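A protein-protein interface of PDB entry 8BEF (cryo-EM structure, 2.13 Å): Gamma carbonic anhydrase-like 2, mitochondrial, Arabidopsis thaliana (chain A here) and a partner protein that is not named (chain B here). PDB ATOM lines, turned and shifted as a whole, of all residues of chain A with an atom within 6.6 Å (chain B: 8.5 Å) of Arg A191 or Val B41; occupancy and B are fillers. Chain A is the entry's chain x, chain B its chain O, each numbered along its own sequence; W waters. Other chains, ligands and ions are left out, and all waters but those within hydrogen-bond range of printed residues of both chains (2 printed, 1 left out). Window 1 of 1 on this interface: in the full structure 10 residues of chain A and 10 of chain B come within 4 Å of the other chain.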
ATOM      1  N   THR A 131      25.670 -36.582  23.762  1.00  0.00           N
ATOM      2  CA  THR A 131      25.081 -36.390  22.442  1.00  0.00           C
ATOM      3  C   THR A 131      25.458 -37.482  21.451  1.00  0.00           C
ATOM      4  O   THR A 131      24.840 -37.563  20.387  1.00  0.00           O
ATOM      5  CB  THR A 131      25.504 -35.037  21.866  1.00  0.00           C
ATOM      6  OG1 THR A 131      26.873 -35.102  21.450  1.00  0.00           O
ATOM      7  CG2 THR A 131      25.354 -33.943  22.910  1.00  0.00           C
ATOM      8  N   LEU A 133      28.133 -37.533  19.685  1.00  0.00           N
ATOM      9  CA  LEU A 133      29.177 -37.008  18.827  1.00  0.00           C
ATOM     10  C   LEU A 133      30.540 -37.241  19.485  1.00  0.00           C
ATOM     11  O   LEU A 133      30.618 -37.455  20.695  1.00  0.00           O
ATOM     12  CB  LEU A 133      28.929 -35.522  18.565  1.00  0.00           C
ATOM     13  CG  LEU A 133      27.715 -35.202  17.690  1.00  0.00           C
ATOM     14  CD1 LEU A 133      27.399 -33.712  17.707  1.00  0.00           C
ATOM     15  CD2 LEU A 133      27.935 -35.696  16.270  1.00  0.00           C
ATOM     16  N   GLY A 171      29.921 -32.320  25.587  1.00  0.00           N
ATOM     17  CA  GLY A 171      29.094 -32.333  24.402  1.00  0.00           C
ATOM     18  C   GLY A 171      28.445 -31.015  24.051  1.00  0.00           C
ATOM     19  O   GLY A 171      27.676 -30.965  23.083  1.00  0.00           O
ATOM     20  N   SER A 172      28.714 -29.952  24.802  1.00  0.00           N
ATOM     21  CA  SER A 172      28.139 -28.655  24.488  1.00  0.00           C
ATOM     22  C   SER A 172      28.795 -28.069  23.239  1.00  0.00           C
ATOM     23  O   SER A 172      29.922 -28.415  22.873  1.00  0.00           O
ATOM     24  CB  SER A 172      28.282 -27.698  25.673  1.00  0.00           C
ATOM     25  OG  SER A 172      29.640 -27.433  25.978  1.00  0.00           O
ATOM     26  N   LEU A 173      28.041 -27.200  22.586  1.00  0.00           N
ATOM     27  CA  LEU A 173      28.483 -26.594  21.313  1.00  0.00           C
ATOM     28  C   LEU A 173      28.240 -25.079  21.221  1.00  0.00           C
ATOM     29  O   LEU A 173      27.179 -24.630  21.498  1.00  0.00           O
ATOM     30  CB  LEU A 173      27.813 -27.341  20.152  1.00  0.00           C
ATOM     31  CG  LEU A 173      27.961 -26.696  18.774  1.00  0.00           C
ATOM     32  CD1 LEU A 173      29.380 -26.891  18.242  1.00  0.00           C
ATOM     33  CD2 LEU A 173      26.933 -27.246  17.802  1.00  0.00           C
ATOM     34  N   VAL A 174      29.277 -24.351  20.932  1.00  0.00           N
ATOM     35  CA  VAL A 174      29.159 -22.911  20.723  1.00  0.00           C
ATOM     36  C   VAL A 174      29.373 -22.649  19.240  1.00  0.00           C
ATOM     37  O   VAL A 174      30.475 -22.848  18.717  1.00  0.00           O
ATOM     38  CB  VAL A 174      30.153 -22.118  21.581  1.00  0.00           C
ATOM     39  CG1 VAL A 174      29.899 -20.629  21.438  1.00  0.00           C
ATOM     40  CG2 VAL A 174      30.040 -22.533  23.036  1.00  0.00           C
ATOM     41  N   GLU A 175      28.299 -22.216  18.606  1.00  0.00           N
ATOM     42  CA  GLU A 175      28.368 -21.966  17.149  1.00  0.00           C
ATOM     43  C   GLU A 175      29.150 -20.681  16.824  1.00  0.00           C
ATOM     44  O   GLU A 175      29.219 -19.821  17.670  1.00  0.00           O
ATOM     45  CB  GLU A 175      26.967 -21.996  16.533  1.00  0.00           C
ATOM     46  CG  GLU A 175      26.248 -23.318  16.685  1.00  0.00           C
ATOM     47  CD  GLU A 175      24.831 -23.318  16.133  1.00  0.00           C
ATOM     48  OE1 GLU A 175      24.393 -22.293  15.555  1.00  0.00           O
ATOM     49  OE2 GLU A 175      24.179 -24.337  16.272  1.00  0.00           O
ATOM     50  N   LEU A 186      27.138 -23.554  30.751  1.00  0.00           N
ATOM     51  CA  LEU A 186      26.479 -24.263  29.664  1.00  0.00           C
ATOM     52  C   LEU A 186      26.375 -25.738  30.018  1.00  0.00           C
ATOM     53  O   LEU A 186      27.401 -26.434  30.034  1.00  0.00           O
ATOM     54  CB  LEU A 186      27.246 -24.080  28.355  1.00  0.00           C
ATOM     55  CG  LEU A 186      26.514 -24.477  27.074  1.00  0.00           C
ATOM     56  CD1 LEU A 186      25.160 -23.789  26.993  1.00  0.00           C
ATOM     57  CD2 LEU A 186      27.354 -24.153  25.852  1.00  0.00           C
ATOM     58  N   PRO A 187      25.184 -26.243  30.357  1.00  0.00           N
ATOM     59  CA  PRO A 187      25.073 -27.637  30.744  1.00  0.00           C
ATOM     60  C   PRO A 187      25.389 -28.637  29.606  1.00  0.00           C
ATOM     61  O   PRO A 187      25.366 -28.290  28.518  1.00  0.00           O
ATOM     62  CB  PRO A 187      23.625 -27.750  31.269  1.00  0.00           C
ATOM     63  CG  PRO A 187      23.181 -26.332  31.528  1.00  0.00           C
ATOM     64  CD  PRO A 187      23.866 -25.573  30.418  1.00  0.00           C
ATOM     65  N   GLY A 189      25.570 -30.990  26.511  1.00  0.00           N
ATOM     66  CA  GLY A 189      24.794 -31.134  25.297  1.00  0.00           C
ATOM     67  C   GLY A 189      24.001 -29.918  24.881  1.00  0.00           C
ATOM     68  O   GLY A 189      23.210 -30.011  23.941  1.00  0.00           O
ATOM     69  N   ARG A 190      24.164 -28.787  25.563  1.00  0.00           N
ATOM     70  CA  ARG A 190      23.467 -27.516  25.248  1.00  0.00           C
ATOM     71  C   ARG A 190      24.211 -26.813  24.098  1.00  0.00           C
ATOM     72  O   ARG A 190      25.361 -27.087  23.877  1.00  0.00           O
ATOM     73  CB  ARG A 190      23.184 -26.629  26.469  1.00  0.00           C
ATOM     74  CG  ARG A 190      21.912 -26.953  27.227  1.00  0.00           C
ATOM     75  CD  ARG A 190      21.867 -28.367  27.752  1.00  0.00           C
ATOM     76  NE  ARG A 190      20.807 -28.569  28.723  1.00  0.00           N
ATOM     77  CZ  ARG A 190      20.736 -29.616  29.538  1.00  0.00           C
ATOM     78  NH1 ARG A 190      21.664 -30.552  29.516  1.00  0.00           N
ATOM     79  NH2 ARG A 190      19.767 -29.690  30.416  1.00  0.00           N
ATOM     80  N   ARG A 191      23.526 -25.946  23.412  1.00  0.00           N
ATOM     81  CA  ARG A 191      24.042 -25.271  22.220  1.00  0.00           C
ATOM     82  C   ARG A 191      23.852 -23.752  22.294  1.00  0.00           C
ATOM     83  O   ARG A 191      22.818 -23.301  22.699  1.00  0.00           O
ATOM     84  CB  ARG A 191      23.372 -25.902  20.990  1.00  0.00           C
ATOM     85  CG  ARG A 191      23.499 -25.174  19.665  1.00  0.00           C
ATOM     86  CD  ARG A 191      22.823 -26.019  18.592  1.00  0.00           C
ATOM     87  NE  ARG A 191      21.379 -26.057  18.657  1.00  0.00           N
ATOM     88  CZ  ARG A 191      20.576 -25.200  18.033  1.00  0.00           C
ATOM     89  NH1 ARG A 191      21.081 -24.231  17.294  1.00  0.00           N
ATOM     90  NH2 ARG A 191      19.276 -25.306  18.174  1.00  0.00           N
ATOM     91  N   ILE A 192      24.830 -23.039  21.858  1.00  0.00           N
ATOM     92  CA  ILE A 192      24.731 -21.592  21.704  1.00  0.00           C
ATOM     93  C   ILE A 192      24.602 -21.298  20.211  1.00  0.00           C
ATOM     94  O   ILE A 192      25.584 -21.469  19.472  1.00  0.00           O
ATOM     95  CB  ILE A 192      25.937 -20.866  22.311  1.00  0.00           C
ATOM     96  CG1 ILE A 192      26.180 -21.325  23.753  1.00  0.00           C
ATOM     97  CG2 ILE A 192      25.726 -19.358  22.256  1.00  0.00           C
ATOM     98  CD1 ILE A 192      25.053 -20.983  24.700  1.00  0.00           C
ATOM     99  N   PRO A 193      23.439 -20.869  19.731  1.00  0.00           N
ATOM    100  CA  PRO A 193      23.269 -20.638  18.290  1.00  0.00           C
ATOM    101  C   PRO A 193      24.122 -19.484  17.785  1.00  0.00           C
ATOM    102  O   PRO A 193      24.427 -18.534  18.510  1.00  0.00           O
ATOM    103  CB  PRO A 193      21.773 -20.325  18.153  1.00  0.00           C
ATOM    104  CG  PRO A 193      21.146 -20.805  19.428  1.00  0.00           C
ATOM    105  CD  PRO A 193      22.193 -20.660  20.481  1.00  0.00           C
ATOM    106  N   SER A 194      24.488 -19.578  16.509  1.00  0.00           N
ATOM    107  CA  SER A 194      25.400 -18.622  15.894  1.00  0.00           C
ATOM    108  C   SER A 194      24.825 -17.209  15.904  1.00  0.00           C
ATOM    109  O   SER A 194      23.619 -17.008  15.741  1.00  0.00           O
ATOM    110  CB  SER A 194      25.709 -19.057  14.459  1.00  0.00           C
ATOM    111  OG  SER A 194      26.399 -18.048  13.744  1.00  0.00           O
ATOM    112  N   TRP A 198      24.789 -14.811  24.863  1.00  0.00           N
ATOM    113  CA  TRP A 198      24.175 -15.622  25.903  1.00  0.00           C
ATOM    114  C   TRP A 198      24.884 -15.378  27.230  1.00  0.00           C
ATOM    115  O   TRP A 198      26.002 -14.860  27.274  1.00  0.00           O
ATOM    116  CB  TRP A 198      24.222 -17.116  25.554  1.00  0.00           C
ATOM    117  CG  TRP A 198      23.178 -17.552  24.580  1.00  0.00           C
ATOM    118  CD1 TRP A 198      22.967 -17.058  23.330  1.00  0.00           C
ATOM    119  CD2 TRP A 198      22.211 -18.594  24.767  1.00  0.00           C
ATOM    120  NE1 TRP A 198      21.922 -17.715  22.731  1.00  0.00           N
ATOM    121  CE2 TRP A 198      21.441 -18.664  23.591  1.00  0.00           C
ATOM    122  CE3 TRP A 198      21.921 -19.470  25.817  1.00  0.00           C
ATOM    123  CZ2 TRP A 198      20.397 -19.575  23.434  1.00  0.00           C
ATOM    124  CZ3 TRP A 198      20.881 -20.370  25.661  1.00  0.00           C
ATOM    125  CH2 TRP A 198      20.136 -20.420  24.477  1.00  0.00           C
ATOM    126  N   GLY B  37      18.724 -26.735  27.666  1.00  0.00           N
ATOM    127  CA  GLY B  37      18.831 -25.305  27.866  1.00  0.00           C
ATOM    128  C   GLY B  37      18.153 -24.592  26.761  1.00  0.00           C
ATOM    129  O   GLY B  37      18.721 -23.564  26.364  1.00  0.00           O
ATOM    130  N   SER B  38      16.982 -25.078  26.336  1.00  0.00           N
ATOM    131  CA  SER B  38      16.101 -24.511  25.317  1.00  0.00           C
ATOM    132  C   SER B  38      16.762 -24.510  23.946  1.00  0.00           C
ATOM    133  O   SER B  38      16.100 -24.265  22.933  1.00  0.00           O
ATOM    134  CB  SER B  38      15.662 -23.093  25.694  1.00  0.00           C
ATOM    135  OG  SER B  38      14.877 -22.514  24.669  1.00  0.00           O
ATOM    136  N   LYS B  39      18.057 -24.813  23.903  1.00  0.00           N
ATOM    137  CA  LYS B  39      18.777 -24.998  22.646  1.00  0.00           C
ATOM    138  C   LYS B  39      19.809 -26.086  22.904  1.00  0.00           C
ATOM    139  O   LYS B  39      20.774 -25.865  23.640  1.00  0.00           O
ATOM    140  CB  LYS B  39      19.438 -23.705  22.168  1.00  0.00           C
ATOM    141  CG  LYS B  39      18.477 -22.616  21.699  1.00  0.00           C
ATOM    142  CD  LYS B  39      17.733 -23.020  20.437  1.00  0.00           C
ATOM    143  CE  LYS B  39      17.047 -21.825  19.789  1.00  0.00           C
ATOM    144  NZ  LYS B  39      15.827 -21.415  20.521  1.00  0.00           N
ATOM    145  N   LYS B  40      19.572 -27.244  22.359  1.00  0.00           N
ATOM    146  CA  LYS B  40      20.419 -28.407  22.499  1.00  0.00           C
ATOM    147  C   LYS B  40      21.037 -28.866  21.182  1.00  0.00           C
ATOM    148  O   LYS B  40      20.447 -28.688  20.118  1.00  0.00           O
ATOM    149  CB  LYS B  40      19.530 -29.526  23.024  1.00  0.00           C
ATOM    150  CG  LYS B  40      18.951 -29.250  24.412  1.00  0.00           C
ATOM    151  CD  LYS B  40      18.113 -30.365  24.951  1.00  0.00           C
ATOM    152  CE  LYS B  40      18.239 -30.630  26.439  1.00  0.00           C
ATOM    153  NZ  LYS B  40      17.672 -29.547  27.267  1.00  0.00           N
ATOM    154  N   VAL B  41      22.124 -29.602  21.326  1.00  0.00           N
ATOM    155  CA  VAL B  41      22.728 -30.244  20.140  1.00  0.00           C
ATOM    156  C   VAL B  41      21.699 -31.276  19.586  1.00  0.00           C
ATOM    157  O   VAL B  41      21.604 -31.420  18.397  1.00  0.00           O
ATOM    158  CB  VAL B  41      24.085 -30.859  20.519  1.00  0.00           C
ATOM    159  CG1 VAL B  41      24.708 -31.611  19.351  1.00  0.00           C
ATOM    160  CG2 VAL B  41      25.059 -29.848  21.109  1.00  0.00           C
ATOM    161  N   SER B  42      20.942 -31.894  20.466  1.00  0.00           N
ATOM    162  CA  SER B  42      19.873 -32.871  20.057  1.00  0.00           C
ATOM    163  C   SER B  42      18.883 -32.242  19.061  1.00  0.00           C
ATOM    164  O   SER B  42      18.534 -32.886  18.187  1.00  0.00           O
ATOM    165  CB  SER B  42      19.210 -33.498  21.255  1.00  0.00           C
ATOM    166  OG  SER B  42      18.748 -32.556  22.183  1.00  0.00           O
ATOM    167  N   ASP B  43      18.681 -30.918  19.117  1.00  0.00           N
ATOM    168  CA  ASP B  43      17.806 -30.216  18.131  1.00  0.00           C
ATOM    169  C   ASP B  43      18.352 -30.320  16.700  1.00  0.00           C
ATOM    170  O   ASP B  43      17.538 -30.177  15.766  1.00  0.00           O
ATOM    171  CB  ASP B  43      17.691 -28.714  18.409  1.00  0.00           C
ATOM    172  CG  ASP B  43      17.290 -28.311  19.819  1.00  0.00           C
ATOM    173  OD1 ASP B  43      16.738 -29.151  20.544  1.00  0.00           O
ATOM    174  OD2 ASP B  43      17.535 -27.143  20.177  1.00  0.00           O
ATOM    175  N   ARG B  44      19.658 -30.549  16.517  1.00  0.00           N
ATOM    176  CA  ARG B  44      20.279 -30.527  15.167  1.00  0.00           C
ATOM    177  C   ARG B  44      20.726 -31.930  14.741  1.00  0.00           C
ATOM    178  O   ARG B  44      21.089 -32.074  13.612  1.00  0.00           O
ATOM    179  CB  ARG B  44      21.460 -29.556  15.176  1.00  0.00           C
ATOM    180  CG  ARG B  44      21.101 -28.084  15.056  1.00  0.00           C
ATOM    181  CD  ARG B  44      22.373 -27.268  15.014  1.00  0.00           C
ATOM    182  NE  ARG B  44      23.176 -27.515  13.829  1.00  0.00           N
ATOM    183  CZ  ARG B  44      24.411 -27.077  13.666  1.00  0.00           C
ATOM    184  NH1 ARG B  44      24.992 -26.404  14.640  1.00  0.00           N
ATOM    185  NH2 ARG B  44      25.074 -27.344  12.557  1.00  0.00           N
ATOM    186  N   ILE B  45      20.645 -32.894  15.621  1.00  0.00           N
ATOM    187  CA  ILE B  45      21.127 -34.270  15.349  1.00  0.00           C
ATOM    188  C   ILE B  45      20.223 -34.927  14.302  1.00  0.00           C
ATOM    189  O   ILE B  45      19.035 -34.792  14.364  1.00  0.00           O
ATOM    190  CB  ILE B  45      21.221 -35.079  16.640  1.00  0.00           C
ATOM    191  CG1 ILE B  45      22.249 -34.523  17.632  1.00  0.00           C
ATOM    192  CG2 ILE B  45      21.417 -36.575  16.377  1.00  0.00           C
ATOM    193  CD1 ILE B  45      23.680 -34.654  17.214  1.00  0.00           C
ATOM    194  N   VAL B  46      20.835 -35.613  13.375  1.00  0.00           N
ATOM    195  CA  VAL B  46      20.063 -36.283  12.298  1.00  0.00           C
ATOM    196  C   VAL B  46      20.383 -37.772  12.345  1.00  0.00           C
ATOM    197  O   VAL B  46      21.583 -38.067  12.242  1.00  0.00           O
ATOM    198  CB  VAL B  46      20.312 -35.619  10.924  1.00  0.00           C
ATOM    199  CG1 VAL B  46      19.649 -36.409   9.803  1.00  0.00           C
ATOM    200  CG2 VAL B  46      19.880 -34.161  10.891  1.00  0.00           C
ATOM    201  N   LYS B  47      19.422 -38.634  12.626  1.00  0.00           N
ATOM    202  CA  LYS B  47      19.611 -40.078  12.712  1.00  0.00           C
ATOM    203  C   LYS B  47      19.851 -40.637  11.314  1.00  0.00           C
ATOM    204  O   LYS B  47      19.105 -40.327  10.381  1.00  0.00           O
ATOM    205  CB  LYS B  47      18.396 -40.752  13.346  1.00  0.00           C
ATOM    206  CG  LYS B  47      18.477 -41.042  14.843  1.00  0.00           C
ATOM    207  CD  LYS B  47      19.420 -40.121  15.575  1.00  0.00           C
ATOM    208  CE  LYS B  47      19.457 -40.443  17.063  1.00  0.00           C
ATOM    209  NZ  LYS B  47      20.294 -39.479  17.830  1.00  0.00           N
ATOM    210  N   ILE B  61      25.512 -40.637  13.341  1.00  0.00           N
ATOM    211  CA  ILE B  61      24.971 -39.382  13.845  1.00  0.00           C
ATOM    212  C   ILE B  61      25.612 -38.227  13.088  1.00  0.00           C
ATOM    213  O   ILE B  61      26.826 -38.228  12.853  1.00  0.00           O
ATOM    214  CB  ILE B  61      25.222 -39.251  15.364  1.00  0.00           C
ATOM    215  CG1 ILE B  61      24.209 -40.087  16.135  1.00  0.00           C
ATOM    216  CG2 ILE B  61      25.110 -37.811  15.813  1.00  0.00           C
ATOM    217  CD1 ILE B  61      22.822 -39.919  15.642  1.00  0.00           C
ATOM    218  N   GLY B  62      24.826 -37.240  12.680  1.00  0.00           N
ATOM    219  CA  GLY B  62      25.397 -35.994  12.160  1.00  0.00           C
ATOM    220  C   GLY B  62      24.570 -34.750  12.497  1.00  0.00           C
ATOM    221  O   GLY B  62      23.401 -34.874  12.741  1.00  0.00           O
ATOM    222  N   LEU B  63      25.164 -33.587  12.406  1.00  0.00           N
ATOM    223  CA  LEU B  63      24.387 -32.326  12.561  1.00  0.00           C
ATOM    224  C   LEU B  63      23.738 -31.851  11.275  1.00  0.00           C
ATOM    225  O   LEU B  63      24.359 -31.939  10.238  1.00  0.00           O
ATOM    226  CB  LEU B  63      25.291 -31.258  13.152  1.00  0.00           C
ATOM    227  CG  LEU B  63      25.878 -31.560  14.530  1.00  0.00           C
ATOM    228  CD1 LEU B  63      26.816 -30.455  14.975  1.00  0.00           C
ATOM    229  CD2 LEU B  63      24.782 -31.786  15.557  1.00  0.00           C
ATOM    230  N   SER B  64      22.515 -31.365  11.399  1.00  0.00           N
ATOM    231  CA  SER B  64      21.826 -30.604  10.353  1.00  0.00           C
ATOM    232  C   SER B  64      22.667 -29.368   9.999  1.00  0.00           C
ATOM    233  O   SER B  64      23.304 -28.809  10.847  1.00  0.00           O
ATOM    234  CB  SER B  64      20.420 -30.162  10.775  1.00  0.00           C
ATOM    235  OG  SER B  64      20.448 -29.505  12.007  1.00  0.00           O
ATOM    236  N   GLN B 141      16.601 -32.062   8.684  1.00  0.00           N
ATOM    237  CA  GLN B 141      15.638 -32.857   9.509  1.00  0.00           C
ATOM    238  C   GLN B 141      14.847 -33.771   8.558  1.00  0.00           C
ATOM    239  O   GLN B 141      14.542 -34.886   8.938  1.00  0.00           O
ATOM    240  CB  GLN B 141      14.798 -31.884  10.396  1.00  0.00           C
ATOM    241  CG  GLN B 141      15.524 -31.329  11.608  1.00  0.00           C
ATOM    242  CD  GLN B 141      16.120 -32.384  12.507  1.00  0.00           C
ATOM    243  OE1 GLN B 141      15.674 -33.526  12.554  1.00  0.00           O
ATOM    244  NE2 GLN B 141      17.159 -32.006  13.225  1.00  0.00           N
HETATM  245  O   HOH W   1      17.374 -30.982  30.340  1.00  0.00           O
HETATM  246  O   HOH W   2      21.875 -32.329  23.243  1.00  0.00           O
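Water W1 bridges NH2 of Arg A190 (2.7 Å) and NZ of Lys B40 (3.4 Å). Water W2 lies within hydrogen-bond range of O of Gly A189, N of Ser B42 and N of Val B41.
Of the printed residues of chain B, Leu A173 touches Val B41 (3.8 Å) and Arg B44 (3.8 Å). Printed residues of chain B within 4 Å of Glu A175: Arg B44. Arg A191 touches just these residues of chain B: Lys B39, Lys B40, Val B41, Asp B43 and Arg B44. Of the printed residues of chain B, Trp A198 touches Gly B37 (3.9 Å) and Lys B39 (3.9 Å). Printed residues of chain A within 4 Å of Lys B40: Gly A189, Arg A190 and Arg A191. Ser B42 touches none of the printed residues of chain A. Of the printed residues of chain A, Ile B45 touches Leu A133. Val B46 touches none of the printed residues of chain A. The nearest residue of chain A that does not touch Val B41 is Thr A131 (4.1 Å).
The backbone NH (N) of Leu A133 sits close to the side-chain hydroxyl (OG1) of Thr A131, at 3.3 Å. The backbone carbonyl oxygen (O) of Leu A173 lies within hydrogen-bond range of the backbone NH (N) of Ile A192, 2.9 Å away. OE2 of Glu A175 is in salt-bridge range of NH1 of Arg A191, at 3.3 Å. The backbone carbonyl oxygen of Ile A192 lies within hydrogen-bond range of the backbone NH of Glu A175 (2.9 Å). OE1 of Glu A175 is in hydrogen-bond range of N of Ser A194. The backbone NH of Ser B64 sits at hydrogen-bond distance from the backbone carbonyl oxygen of Arg B44.
Of the 16 printed residues of chain A, 9 touch a printed residue of chain B. Printed residues of chain A that touch a printed residue of chain B: Leu A133, Gly A171, Leu A173, Glu A175, Gly A189, Arg A190, Arg A191, Pro A193 and Trp A198. Hydrophobic or aromatic side chains of chain A that line the printed part of chain B: Leu A133, Leu A173, Pro A193 and Trp A198. Printed residues of chain B that touch a printed residue of chain A: Gly B37, Lys B39, Lys B40, Val B41, Asp B43, Arg B44, Ile B45, Ile B61 and Leu B63. Along chain B the printed residues that touch a printed residue of chain A span positions 37 to 63. Among the printed residues, Asp or Glu carboxylates within 4 Å of a Lys or Arg side-chain nitrogen of the other chain: Glu A175 with Arg B44 (2.8 Å) and Arg A191 with Asp B43 (3.2 Å).
The side-chain carboxylate (OE2) of Glu A175 is in salt-bridge range of the guanidinium group (NH1) of Arg B44 (2.8 Å). N of Val B41 sits at hydrogen-bond distance from O of Gly A189, 2.9 Å away. The backbone carbonyl oxygen (O) of Lys B39 is in hydrogen-bond range of the backbone NH (N) of Arg A191, at 2.8 Å. The guanidinium group (NE) of Arg A191 lies within hydrogen-bond range of the backbone carbonyl oxygen (O) of Lys B40, 3.2 Å away. NH2 of Arg A191 is in salt-bridge range of OD2 of Asp B43 (3.2 Å). NE of Arg A190 sits close to N of Gly B37 (3.0 Å).
Leu A133 touches Val B41. CD1 of Ile B45 touches CD1 of Leu A133, 3.9 Å away. CD2 of Leu A133 touches CG2 of Ile B61, at 3.6 Å. Leu A133 touches Leu B63. CG2 of Val B41 touches O of Gly A171, at 3.5 Å. CG2 of Val B41 touches CB of Leu A173, at 3.8 Å. Leu A173 touches Arg B44. CA of Arg A190 touches O of Lys B39, at 3.5 Å. Val B41 touches Arg A191. Lys B39 touches Trp A198 (CG to CH2, 3.9 Å).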
